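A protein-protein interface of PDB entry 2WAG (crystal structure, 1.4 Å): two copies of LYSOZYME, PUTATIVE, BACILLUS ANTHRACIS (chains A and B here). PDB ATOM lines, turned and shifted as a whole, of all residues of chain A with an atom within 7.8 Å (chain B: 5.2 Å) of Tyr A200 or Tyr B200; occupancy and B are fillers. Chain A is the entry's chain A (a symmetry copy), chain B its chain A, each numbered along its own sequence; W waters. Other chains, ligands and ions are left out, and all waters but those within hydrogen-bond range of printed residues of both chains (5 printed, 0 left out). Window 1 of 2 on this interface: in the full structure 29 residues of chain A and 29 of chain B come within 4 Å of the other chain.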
ATOM      1  N   GLY A   2      -7.949   0.846 -31.058  1.00  0.00           N
ATOM      2  CA  GLY A   2      -6.489   0.747 -30.803  1.00  0.00           C
ATOM      3  C   GLY A   2      -6.201   1.352 -29.453  1.00  0.00           C
ATOM      4  O   GLY A   2      -7.126   1.685 -28.695  1.00  0.00           O
ATOM      5  N   SER A   3      -4.924   1.483 -29.144  1.00  0.00           N
ATOM      6  CA  SER A   3      -4.510   1.827 -27.786  1.00  0.00           C
ATOM      7  C   SER A   3      -3.747   3.134 -27.755  1.00  0.00           C
ATOM      8  O   SER A   3      -2.773   3.295 -28.515  1.00  0.00           O
ATOM      9  CB  SER A   3      -3.561   0.757 -27.265  1.00  0.00           C
ATOM     10  OG  SER A   3      -4.199  -0.488 -27.165  1.00  0.00           O
ATOM     11  N   SER A   4      -4.150   4.037 -26.863  1.00  0.00           N
ATOM     12  CA  SER A   4      -3.402   5.263 -26.608  1.00  0.00           C
ATOM     13  C   SER A   4      -2.389   5.053 -25.493  1.00  0.00           C
ATOM     14  O   SER A   4      -2.628   4.260 -24.571  1.00  0.00           O
ATOM     15  CB  SER A   4      -4.357   6.364 -26.168  1.00  0.00           C
ATOM     16  OG  SER A   4      -3.658   7.557 -25.816  1.00  0.00           O
ATOM     17  N   ASP A  20     -10.443  -4.363  -9.580  1.00  0.00           N
ATOM     18  CA  ASP A  20     -11.302  -5.536  -9.746  1.00  0.00           C
ATOM     19  C   ASP A  20     -10.601  -6.433 -10.740  1.00  0.00           C
ATOM     20  O   ASP A  20      -9.976  -5.928 -11.671  1.00  0.00           O
ATOM     21  CB  ASP A  20     -12.752  -5.196 -10.151  1.00  0.00           C
ATOM     22  CG  ASP A  20     -12.851  -4.571 -11.495  1.00  0.00           C
ATOM     23  OD1 ASP A  20     -12.841  -3.345 -11.534  1.00  0.00           O
ATOM     24  OD2 ASP A  20     -12.946  -5.299 -12.495  1.00  0.00           O
ATOM     25  N   VAL A  21     -10.652  -7.736 -10.497  1.00  0.00           N
ATOM     26  CA  VAL A  21      -9.925  -8.694 -11.310  1.00  0.00           C
ATOM     27  C   VAL A  21     -10.730  -9.958 -11.546  1.00  0.00           C
ATOM     28  O   VAL A  21     -11.642 -10.289 -10.769  1.00  0.00           O
ATOM     29  CB  VAL A  21      -8.564  -9.110 -10.661  1.00  0.00           C
ATOM     30  CG1 VAL A  21      -7.679  -7.894 -10.417  1.00  0.00           C
ATOM     31  CG2 VAL A  21      -8.788  -9.914  -9.384  1.00  0.00           C
ATOM     32  N   ALA A  22     -10.356 -10.666 -12.607  1.00  0.00           N
ATOM     33  CA  ALA A  22     -10.849 -12.004 -12.911  1.00  0.00           C
ATOM     34  C   ALA A  22      -9.645 -12.827 -13.331  1.00  0.00           C
ATOM     35  O   ALA A  22      -8.493 -12.345 -13.284  1.00  0.00           O
ATOM     36  CB  ALA A  22     -11.900 -11.951 -14.021  1.00  0.00           C
ATOM     37  N   SER A  23      -9.879 -14.066 -13.756  1.00  0.00           N
ATOM     38  CA  SER A  23      -8.749 -14.918 -14.107  1.00  0.00           C
ATOM     39  C   SER A  23      -7.903 -14.334 -15.236  1.00  0.00           C
ATOM     40  O   SER A  23      -6.715 -14.626 -15.313  1.00  0.00           O
ATOM     41  CB  SER A  23      -9.226 -16.321 -14.484  1.00  0.00           C
ATOM     42  OG  SER A  23     -10.058 -16.268 -15.629  1.00  0.00           O
ATOM     43  N   TYR A  24      -8.508 -13.502 -16.089  1.00  0.00           N
ATOM     44  CA  TYR A  24      -7.810 -12.942 -17.268  1.00  0.00           C
ATOM     45  C   TYR A  24      -6.668 -12.035 -16.867  1.00  0.00           C
ATOM     46  O   TYR A  24      -5.812 -11.755 -17.692  1.00  0.00           O
ATOM     47  CB  TYR A  24      -8.823 -12.260 -18.232  1.00  0.00           C
ATOM     48  CG  TYR A  24     -10.005 -13.180 -18.355  1.00  0.00           C
ATOM     49  CD1 TYR A  24      -9.842 -14.480 -18.859  1.00  0.00           C
ATOM     50  CD2 TYR A  24     -11.229 -12.844 -17.813  1.00  0.00           C
ATOM     51  CE1 TYR A  24     -10.886 -15.373 -18.867  1.00  0.00           C
ATOM     52  CE2 TYR A  24     -12.280 -13.734 -17.834  1.00  0.00           C
ATOM     53  CZ  TYR A  24     -12.097 -14.997 -18.342  1.00  0.00           C
ATOM     54  OH  TYR A  24     -13.151 -15.882 -18.318  1.00  0.00           O
ATOM     55  N   GLN A  25      -6.662 -11.553 -15.623  1.00  0.00           N
ATOM     56  CA  GLN A  25      -5.559 -10.742 -15.119  1.00  0.00           C
ATOM     57  C   GLN A  25      -4.358 -11.598 -14.690  1.00  0.00           C
ATOM     58  O   GLN A  25      -3.333 -11.059 -14.263  1.00  0.00           O
ATOM     59  CB  GLN A  25      -6.025  -9.826 -13.973  1.00  0.00           C
ATOM     60  CG  GLN A  25      -6.707  -8.559 -14.466  1.00  0.00           C
ATOM     61  CD  GLN A  25      -7.923  -8.840 -15.328  1.00  0.00           C
ATOM     62  OE1 GLN A  25      -8.867  -9.524 -14.895  1.00  0.00           O
ATOM     63  NE2 GLN A  25      -7.902  -8.344 -16.578  1.00  0.00           N
ATOM     64  N   GLY A  26      -4.493 -12.924 -14.756  1.00  0.00           N
ATOM     65  CA  GLY A  26      -3.352 -13.810 -14.487  1.00  0.00           C
ATOM     66  C   GLY A  26      -2.986 -13.875 -13.016  1.00  0.00           C
ATOM     67  O   GLY A  26      -3.833 -13.697 -12.138  1.00  0.00           O
ATOM     68  N   THR A 186     -10.767   3.133 -15.376  1.00  0.00           N
ATOM     69  CA  THR A 186      -9.896   2.668 -16.455  1.00  0.00           C
ATOM     70  C   THR A 186      -9.887   1.157 -16.502  1.00  0.00           C
ATOM     71  O   THR A 186     -10.121   0.500 -15.477  1.00  0.00           O
ATOM     72  CB  THR A 186      -8.443   3.188 -16.297  1.00  0.00           C
ATOM     73  OG1 THR A 186      -7.675   2.789 -17.450  1.00  0.00           O
ATOM     74  CG2 THR A 186      -7.777   2.645 -15.047  1.00  0.00           C
ATOM     75  N   ASN A 187      -9.662   0.629 -17.704  1.00  0.00           N
ATOM     76  CA  ASN A 187      -9.458  -0.802 -17.955  1.00  0.00           C
ATOM     77  C   ASN A 187      -7.991  -1.169 -18.027  1.00  0.00           C
ATOM     78  O   ASN A 187      -7.638  -2.349 -18.052  1.00  0.00           O
ATOM     79  CB  ASN A 187     -10.081  -1.218 -19.291  1.00  0.00           C
ATOM     80  CG  ASN A 187      -9.453  -0.509 -20.467  1.00  0.00           C
ATOM     81  OD1 ASN A 187      -9.408   0.731 -20.497  1.00  0.00           O
ATOM     82  ND2 ASN A 187      -8.965  -1.283 -21.456  1.00  0.00           N
ATOM     83  N   ARG A 188      -7.128  -0.173 -18.147  1.00  0.00           N
ATOM     84  CA  ARG A 188      -5.706  -0.444 -18.302  1.00  0.00           C
ATOM     85  C   ARG A 188      -4.949   0.359 -17.269  1.00  0.00           C
ATOM     86  O   ARG A 188      -4.257   1.321 -17.603  1.00  0.00           O
ATOM     87  CB  ARG A 188      -5.236  -0.073 -19.708  1.00  0.00           C
ATOM     88  CG  ARG A 188      -3.964  -0.781 -20.144  1.00  0.00           C
ATOM     89  CD  ARG A 188      -3.549  -0.359 -21.544  1.00  0.00           C
ATOM     90  NE  ARG A 188      -2.691   0.822 -21.528  1.00  0.00           N
ATOM     91  CZ  ARG A 188      -2.793   1.832 -22.385  1.00  0.00           C
ATOM     92  NH1 ARG A 188      -1.969   2.868 -22.295  1.00  0.00           N
ATOM     93  NH2 ARG A 188      -3.720   1.809 -23.332  1.00  0.00           N
ATOM     94  N   GLY A 189      -5.091  -0.027 -16.007  1.00  0.00           N
ATOM     95  CA  GLY A 189      -4.557   0.776 -14.969  1.00  0.00           C
ATOM     96  C   GLY A 189      -3.060   0.963 -15.101  1.00  0.00           C
ATOM     97  O   GLY A 189      -2.293   0.135 -15.478  1.00  0.00           O
ATOM     98  N   LEU A 191       0.389   1.291 -13.341  1.00  0.00           N
ATOM     99  CA  LEU A 191       1.104   0.490 -12.214  1.00  0.00           C
ATOM    100  C   LEU A 191       2.639   0.649 -12.072  1.00  0.00           C
ATOM    101  O   LEU A 191       3.402   0.508 -12.963  1.00  0.00           O
ATOM    102  CB  LEU A 191       0.896  -1.060 -12.173  1.00  0.00           C
ATOM    103  CG  LEU A 191      -0.511  -1.653 -12.292  1.00  0.00           C
ATOM    104  CD1 LEU A 191      -0.679  -3.111 -12.020  1.00  0.00           C
ATOM    105  CD2 LEU A 191      -1.357  -0.893 -11.411  1.00  0.00           C
ATOM    106  N   LYS A 197       4.360  -2.385 -14.800  1.00  0.00           N
ATOM    107  CA  LYS A 197       4.241  -2.214 -16.239  1.00  0.00           C
ATOM    108  C   LYS A 197       2.817  -1.800 -16.535  1.00  0.00           C
ATOM    109  O   LYS A 197       1.970  -1.711 -15.632  1.00  0.00           O
ATOM    110  CB  LYS A 197       4.564  -3.514 -16.986  1.00  0.00           C
ATOM    111  CG  LYS A 197       3.940  -4.755 -16.391  1.00  0.00           C
ATOM    112  CD  LYS A 197       4.794  -5.962 -16.737  1.00  0.00           C
ATOM    113  CE  LYS A 197       4.276  -6.639 -17.979  1.00  0.00           C
ATOM    114  NZ  LYS A 197       3.285  -7.699 -17.635  1.00  0.00           N
ATOM    115  N   GLU A 198       2.553  -1.539 -17.805  1.00  0.00           N
ATOM    116  CA  GLU A 198       1.187  -1.335 -18.255  1.00  0.00           C
ATOM    117  C   GLU A 198       0.464  -2.675 -18.104  1.00  0.00           C
ATOM    118  O   GLU A 198       0.958  -3.714 -18.544  1.00  0.00           O
ATOM    119  CB  GLU A 198       1.199  -0.888 -19.715  1.00  0.00           C
ATOM    120  CG  GLU A 198       1.757   0.523 -19.946  1.00  0.00           C
ATOM    121  CD  GLU A 198       0.712   1.610 -19.828  1.00  0.00           C
ATOM    122  OE1 GLU A 198      -0.486   1.298 -19.613  1.00  0.00           O
ATOM    123  OE2 GLU A 198       1.095   2.790 -19.977  1.00  0.00           O
ATOM    124  N   LYS A 199      -0.686  -2.683 -17.436  1.00  0.00           N
ATOM    125  CA  LYS A 199      -1.398  -3.951 -17.259  1.00  0.00           C
ATOM    126  C   LYS A 199      -2.882  -3.787 -17.592  1.00  0.00           C
ATOM    127  O   LYS A 199      -3.467  -2.744 -17.247  1.00  0.00           O
ATOM    128  CB  LYS A 199      -1.227  -4.478 -15.811  1.00  0.00           C
ATOM    129  CG  LYS A 199      -1.961  -5.791 -15.661  1.00  0.00           C
ATOM    130  CD  LYS A 199      -1.799  -6.350 -14.276  1.00  0.00           C
ATOM    131  CE  LYS A 199      -2.563  -7.659 -14.118  1.00  0.00           C
ATOM    132  NZ  LYS A 199      -2.094  -8.706 -15.078  1.00  0.00           N
ATOM    133  N   TYR A 200      -3.512  -4.810 -18.201  1.00  0.00           N
ATOM    134  CA  TYR A 200      -4.989  -4.779 -18.347  1.00  0.00           C
ATOM    135  C   TYR A 200      -5.582  -5.225 -17.042  1.00  0.00           C
ATOM    136  O   TYR A 200      -5.684  -6.431 -16.791  1.00  0.00           O
ATOM    137  CB  TYR A 200      -5.496  -5.623 -19.531  1.00  0.00           C
ATOM    138  CG  TYR A 200      -5.171  -4.950 -20.846  1.00  0.00           C
ATOM    139  CD1 TYR A 200      -5.988  -3.950 -21.362  1.00  0.00           C
ATOM    140  CD2 TYR A 200      -4.045  -5.314 -21.569  1.00  0.00           C
ATOM    141  CE1 TYR A 200      -5.663  -3.313 -22.577  1.00  0.00           C
ATOM    142  CE2 TYR A 200      -3.733  -4.695 -22.764  1.00  0.00           C
ATOM    143  CZ  TYR A 200      -4.534  -3.711 -23.269  1.00  0.00           C
ATOM    144  OH  TYR A 200      -4.201  -3.102 -24.464  1.00  0.00           O
ATOM    145  N   ILE A 201      -5.796  -4.243 -16.168  1.00  0.00           N
ATOM    146  CA  ILE A 201      -6.450  -4.433 -14.899  1.00  0.00           C
ATOM    147  C   ILE A 201      -7.299  -3.200 -14.634  1.00  0.00           C
ATOM    148  O   ILE A 201      -6.878  -2.058 -14.847  1.00  0.00           O
ATOM    149  CB  ILE A 201      -5.429  -4.608 -13.789  1.00  0.00           C
ATOM    150  CG1 ILE A 201      -6.122  -4.986 -12.472  1.00  0.00           C
ATOM    151  CG2 ILE A 201      -4.538  -3.359 -13.703  1.00  0.00           C
ATOM    152  CD1 ILE A 201      -5.146  -5.444 -11.433  1.00  0.00           C
ATOM    153  N   ASP A 202      -8.530  -3.440 -14.215  1.00  0.00           N
ATOM    154  CA  ASP A 202      -9.484  -2.383 -13.940  1.00  0.00           C
ATOM    155  C   ASP A 202      -9.180  -1.649 -12.633  1.00  0.00           C
ATOM    156  O   ASP A 202      -8.967  -2.292 -11.597  1.00  0.00           O
ATOM    157  CB  ASP A 202     -10.871  -3.007 -13.737  1.00  0.00           C
ATOM    158  CG  ASP A 202     -11.458  -3.622 -15.008  1.00  0.00           C
ATOM    159  OD1 ASP A 202     -11.070  -3.237 -16.137  1.00  0.00           O
ATOM    160  OD2 ASP A 202     -12.357  -4.495 -14.860  1.00  0.00           O
ATOM    161  N   LEU A 203      -9.218  -0.335 -12.706  1.00  0.00           N
ATOM    162  CA  LEU A 203      -9.062   0.500 -11.510  1.00  0.00           C
ATOM    163  C   LEU A 203     -10.286   1.315 -11.225  1.00  0.00           C
ATOM    164  O   LEU A 203     -10.987   1.729 -12.087  1.00  0.00           O
ATOM    165  CB  LEU A 203      -7.820   1.416 -11.568  1.00  0.00           C
ATOM    166  CG  LEU A 203      -6.475   0.726 -11.911  1.00  0.00           C
ATOM    167  CD1 LEU A 203      -5.385   1.808 -11.900  1.00  0.00           C
ATOM    168  CD2 LEU A 203      -6.143  -0.358 -10.983  1.00  0.00           C
ATOM    169  N   SER B   3     -15.526  -9.063 -16.269  1.00  0.00           N
ATOM    170  CA  SER B   3     -15.172  -9.910 -17.406  1.00  0.00           C
ATOM    171  C   SER B   3     -16.044 -11.146 -17.469  1.00  0.00           C
ATOM    172  O   SER B   3     -16.157 -11.869 -16.461  1.00  0.00           O
ATOM    173  CB  SER B   3     -13.740 -10.397 -17.242  1.00  0.00           C
ATOM    174  OG  SER B   3     -12.830  -9.329 -17.263  1.00  0.00           O
ATOM    175  N   TYR B  24       1.263  -2.711 -25.522  1.00  0.00           N
ATOM    176  CA  TYR B  24       0.554  -3.264 -24.346  1.00  0.00           C
ATOM    177  C   TYR B  24       0.292  -4.748 -24.493  1.00  0.00           C
ATOM    178  O   TYR B  24       0.013  -5.403 -23.502  1.00  0.00           O
ATOM    179  CB  TYR B  24      -0.732  -2.443 -24.044  1.00  0.00           C
ATOM    180  CG  TYR B  24      -0.365  -0.989 -24.155  1.00  0.00           C
ATOM    181  CD1 TYR B  24       0.621  -0.441 -23.321  1.00  0.00           C
ATOM    182  CD2 TYR B  24      -0.847  -0.210 -25.188  1.00  0.00           C
ATOM    183  CE1 TYR B  24       1.052   0.853 -23.489  1.00  0.00           C
ATOM    184  CE2 TYR B  24      -0.425   1.090 -25.349  1.00  0.00           C
ATOM    185  CZ  TYR B  24       0.534   1.607 -24.512  1.00  0.00           C
ATOM    186  OH  TYR B  24       0.967   2.897 -24.715  1.00  0.00           O
ATOM    187  N   GLN B  25       0.352  -5.272 -25.718  1.00  0.00           N
ATOM    188  CA  GLN B  25       0.200  -6.704 -25.948  1.00  0.00           C
ATOM    189  C   GLN B  25       1.494  -7.479 -25.659  1.00  0.00           C
ATOM    190  O   GLN B  25       1.522  -8.706 -25.783  1.00  0.00           O
ATOM    191  CB  GLN B  25      -0.308  -6.983 -27.375  1.00  0.00           C
ATOM    192  CG  GLN B  25      -1.813  -6.820 -27.512  1.00  0.00           C
ATOM    193  CD  GLN B  25      -2.293  -5.432 -27.139  1.00  0.00           C
ATOM    194  OE1 GLN B  25      -1.842  -4.424 -27.713  1.00  0.00           O
ATOM    195  NE2 GLN B  25      -3.194  -5.352 -26.141  1.00  0.00           N
ATOM    196  N   ASN B 187     -11.960  -7.443 -28.047  1.00  0.00           N
ATOM    197  CA  ASN B 187     -10.751  -6.936 -27.389  1.00  0.00           C
ATOM    198  C   ASN B 187      -9.984  -8.029 -26.674  1.00  0.00           C
ATOM    199  O   ASN B 187      -8.859  -7.816 -26.222  1.00  0.00           O
ATOM    200  CB  ASN B 187     -11.102  -5.883 -26.333  1.00  0.00           C
ATOM    201  CG  ASN B 187     -11.962  -6.442 -25.224  1.00  0.00           C
ATOM    202  OD1 ASN B 187     -13.032  -7.011 -25.489  1.00  0.00           O
ATOM    203  ND2 ASN B 187     -11.511  -6.281 -23.964  1.00  0.00           N
ATOM    204  N   ARG B 188     -10.613  -9.179 -26.486  1.00  0.00           N
ATOM    205  CA  ARG B 188      -9.977 -10.253 -25.739  1.00  0.00           C
ATOM    206  C   ARG B 188     -10.032 -11.514 -26.569  1.00  0.00           C
ATOM    207  O   ARG B 188     -10.768 -12.448 -26.248  1.00  0.00           O
ATOM    208  CB  ARG B 188     -10.682 -10.470 -24.400  1.00  0.00           C
ATOM    209  CG  ARG B 188      -9.823 -11.156 -23.350  1.00  0.00           C
ATOM    210  CD  ARG B 188     -10.588 -11.349 -22.051  1.00  0.00           C
ATOM    211  NE  ARG B 188     -11.326 -12.609 -22.033  1.00  0.00           N
ATOM    212  CZ  ARG B 188     -12.560 -12.745 -21.561  1.00  0.00           C
ATOM    213  NH1 ARG B 188     -13.154 -13.931 -21.585  1.00  0.00           N
ATOM    214  NH2 ARG B 188     -13.202 -11.697 -21.065  1.00  0.00           N
ATOM    215  N   GLU B 198      -6.162 -17.052 -22.758  1.00  0.00           N
ATOM    216  CA  GLU B 198      -6.952 -15.845 -22.929  1.00  0.00           C
ATOM    217  C   GLU B 198      -5.969 -14.675 -23.006  1.00  0.00           C
ATOM    218  O   GLU B 198      -5.077 -14.543 -22.167  1.00  0.00           O
ATOM    219  CB  GLU B 198      -7.892 -15.686 -21.736  1.00  0.00           C
ATOM    220  CG  GLU B 198      -9.022 -16.724 -21.670  1.00  0.00           C
ATOM    221  CD  GLU B 198     -10.256 -16.320 -22.445  1.00  0.00           C
ATOM    222  OE1 GLU B 198     -10.292 -15.202 -23.016  1.00  0.00           O
ATOM    223  OE2 GLU B 198     -11.210 -17.128 -22.460  1.00  0.00           O
ATOM    224  N   LYS B 199      -6.080 -13.843 -24.037  1.00  0.00           N
ATOM    225  CA  LYS B 199      -5.147 -12.721 -24.150  1.00  0.00           C
ATOM    226  C   LYS B 199      -5.896 -11.424 -24.460  1.00  0.00           C
ATOM    227  O   LYS B 199      -6.858 -11.456 -25.250  1.00  0.00           O
ATOM    228  CB  LYS B 199      -4.083 -13.000 -25.242  1.00  0.00           C
ATOM    229  CG  LYS B 199      -3.127 -11.833 -25.329  1.00  0.00           C
ATOM    230  CD  LYS B 199      -2.062 -12.076 -26.360  1.00  0.00           C
ATOM    231  CE  LYS B 199      -1.117 -10.885 -26.466  1.00  0.00           C
ATOM    232  NZ  LYS B 199      -0.424 -10.598 -25.171  1.00  0.00           N
ATOM    233  N   TYR B 200      -5.447 -10.282 -23.903  1.00  0.00           N
ATOM    234  CA  TYR B 200      -6.008  -8.981 -24.344  1.00  0.00           C
ATOM    235  C   TYR B 200      -5.318  -8.599 -25.621  1.00  0.00           C
ATOM    236  O   TYR B 200      -4.211  -8.050 -25.583  1.00  0.00           O
ATOM    237  CB  TYR B 200      -5.894  -7.881 -23.274  1.00  0.00           C
ATOM    238  CG  TYR B 200      -6.872  -8.126 -22.146  1.00  0.00           C
ATOM    239  CD1 TYR B 200      -8.200  -7.724 -22.247  1.00  0.00           C
ATOM    240  CD2 TYR B 200      -6.468  -8.763 -20.983  1.00  0.00           C
ATOM    241  CE1 TYR B 200      -9.110  -7.979 -21.202  1.00  0.00           C
ATOM    242  CE2 TYR B 200      -7.359  -9.004 -19.955  1.00  0.00           C
ATOM    243  CZ  TYR B 200      -8.663  -8.611 -20.056  1.00  0.00           C
ATOM    244  OH  TYR B 200      -9.538  -8.866 -19.016  1.00  0.00           O
ATOM    245  N   ILE B 201      -5.904  -9.058 -26.725  1.00  0.00           N
ATOM    246  CA  ILE B 201      -5.466  -8.726 -28.057  1.00  0.00           C
ATOM    247  C   ILE B 201      -6.709  -8.592 -28.924  1.00  0.00           C
ATOM    248  O   ILE B 201      -7.642  -9.399 -28.859  1.00  0.00           O
ATOM    249  CB  ILE B 201      -4.561  -9.811 -28.612  1.00  0.00           C
ATOM    250  CG1 ILE B 201      -3.956  -9.375 -29.954  1.00  0.00           C
ATOM    251  CG2 ILE B 201      -5.321 -11.146 -28.661  1.00  0.00           C
ATOM    252  CD1 ILE B 201      -2.847 -10.280 -30.393  1.00  0.00           C
ATOM    253  N   ASP B 202      -6.740  -7.527 -29.707  1.00  0.00           N
ATOM    254  CA  ASP B 202      -7.859  -7.228 -30.579  1.00  0.00           C
ATOM    255  C   ASP B 202      -7.898  -8.135 -31.809  1.00  0.00           C
ATOM    256  O   ASP B 202      -6.878  -8.300 -32.490  1.00  0.00           O
ATOM    257  CB  ASP B 202      -7.692  -5.807 -31.132  1.00  0.00           C
ATOM    258  CG  ASP B 202      -7.834  -4.716 -30.072  1.00  0.00           C
ATOM    259  OD1 ASP B 202      -8.472  -4.937 -29.015  1.00  0.00           O
ATOM    260  OD2 ASP B 202      -7.314  -3.596 -30.329  1.00  0.00           O
HETATM  261  O   HOH W   1      -3.878  -2.815 -28.491  1.00  0.00           O
HETATM  262  O   HOH W   2     -11.217  -8.266 -15.380  1.00  0.00           O
HETATM  263  O   HOH W   3      -9.119  -1.188 -29.553  1.00  0.00           O
HETATM  264  O   HOH W   4      -6.666  -2.866 -27.242  1.00  0.00           O
HETATM  265  O   HOH W   5     -11.601  -6.141 -17.542  1.00  0.00           O
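Printed residues of chain A that touch a printed residue of chain B: Ser A3, Ser A4, Tyr A24, Gln A25, Arg A188, Glu A198 and Tyr A200. Of the 10 printed residues of chain B, 6 touch a printed residue of chain A.
Water W1 bridges the side-chain hydroxyl of Ser A3 (2.7 Å) and the side-chain amide oxygen of Gln B25 (2.7 Å). Water W2 bridges OG of Ser B3 and OE1 of Gln A25. Water W3 lies within hydrogen-bond range of the backbone NH of Gly A2 (2.8 Å) and the side-chain carboxylate of Asp B202 (3.1 Å). Water W5 bridges the side-chain carboxylate of Asp A202 and the side-chain hydroxyl of Ser B3. Water W4 bridges the side-chain carboxylate (OD2) of Asp B202 (3.2 Å) and the side-chain hydroxyl (OG) of Ser A3 (3.4 Å).
Tyr B24 touches Ser A3. Tyr B24 touches Ser A4. Ser B3 touches Tyr A24. NH1 of Arg B188 touches CZ of Tyr A24 (3.6 Å). Tyr A24 touches Glu B198 (CE1 to CG, 3.6 Å). OH of Tyr B200 touches CB of Tyr A24, 3.6 Å away. Tyr B24 touches Arg A188 (CZ to NH1, 3.6 Å). Glu A198 touches Tyr B24. Tyr B24 touches Tyr A200 (CB to OH, 3.6 Å). Tyr A200 touches Tyr B200.
The side-chain amino group (NZ) of Lys B199 sits at hydrogen-bond distance from the backbone carbonyl oxygen (O) of Gln B25, 2.8 Å away. O of Ser A4 lies within hydrogen-bond range of NH1 of Arg A188 (2.7 Å). N of Ala A22 is in hydrogen-bond range of OE1 of Gln A25 (3.0 Å). O of Gln A25 lies within hydrogen-bond range of NZ of Lys A199, at 2.8 Å. N of Arg A188 sits at hydrogen-bond distance from OG1 of Thr A186, 3.1 Å away. The side-chain carboxylate (OE1) of Glu A198 lies within salt-bridge range of the guanidinium group (NE) of Arg A188 (3.0 Å).
NE2 of Gln B25 sits at hydrogen-bond distance from OH of Tyr A200. The side-chain hydroxyl of Tyr B200 lies within hydrogen-bond range of the side-chain amide nitrogen of Gln A25, 3.0 Å away.
Tyr A200 touches three residues of chain B. Tyr B200 touches three residues of chain A. Of the printed residues of chain B, Ser A4 touches Tyr B24. Printed residues of chain A within 4 Å of Glu B198: Tyr A24. Of the printed residues of chain A, Arg B188 touches Tyr A24. Printed residues of chain B within 4 Å of Arg A188: Tyr B24 (3.6 Å). Lys A197 touches none of the printed residues of chain B. Asp A20 touches none of the printed residues of chain B. The nearest printed residue of chain B that does not touch Tyr A200 is Ile B201 (6.3 Å). The nearest printed residue of chain A that does not touch Tyr B200 is Ile A201 (6.3 Å). The nearest printed residue of chain A that does not touch Tyr B24 is Lys A199 (6.4 Å).
Tyr A24 touches Glu B198, and with the chains exchanged Glu A198 touches Tyr B24. Tyr A24 touches Tyr B200, and with the chains exchanged Tyr A200 touches Tyr B24. Gln A25 touches Tyr B200, and with the chains exchanged Tyr A200 touches Gln B25. Tyr A200 touches its own counterpart, Tyr B200. Positions printed for both chains: 3, 24, 25, 187, 188, 198, 199, 200, 201 and 202. Of the 12 pairs that touch across the chains among the printed residues, 11 have their exchanged pair printed and touching as well.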
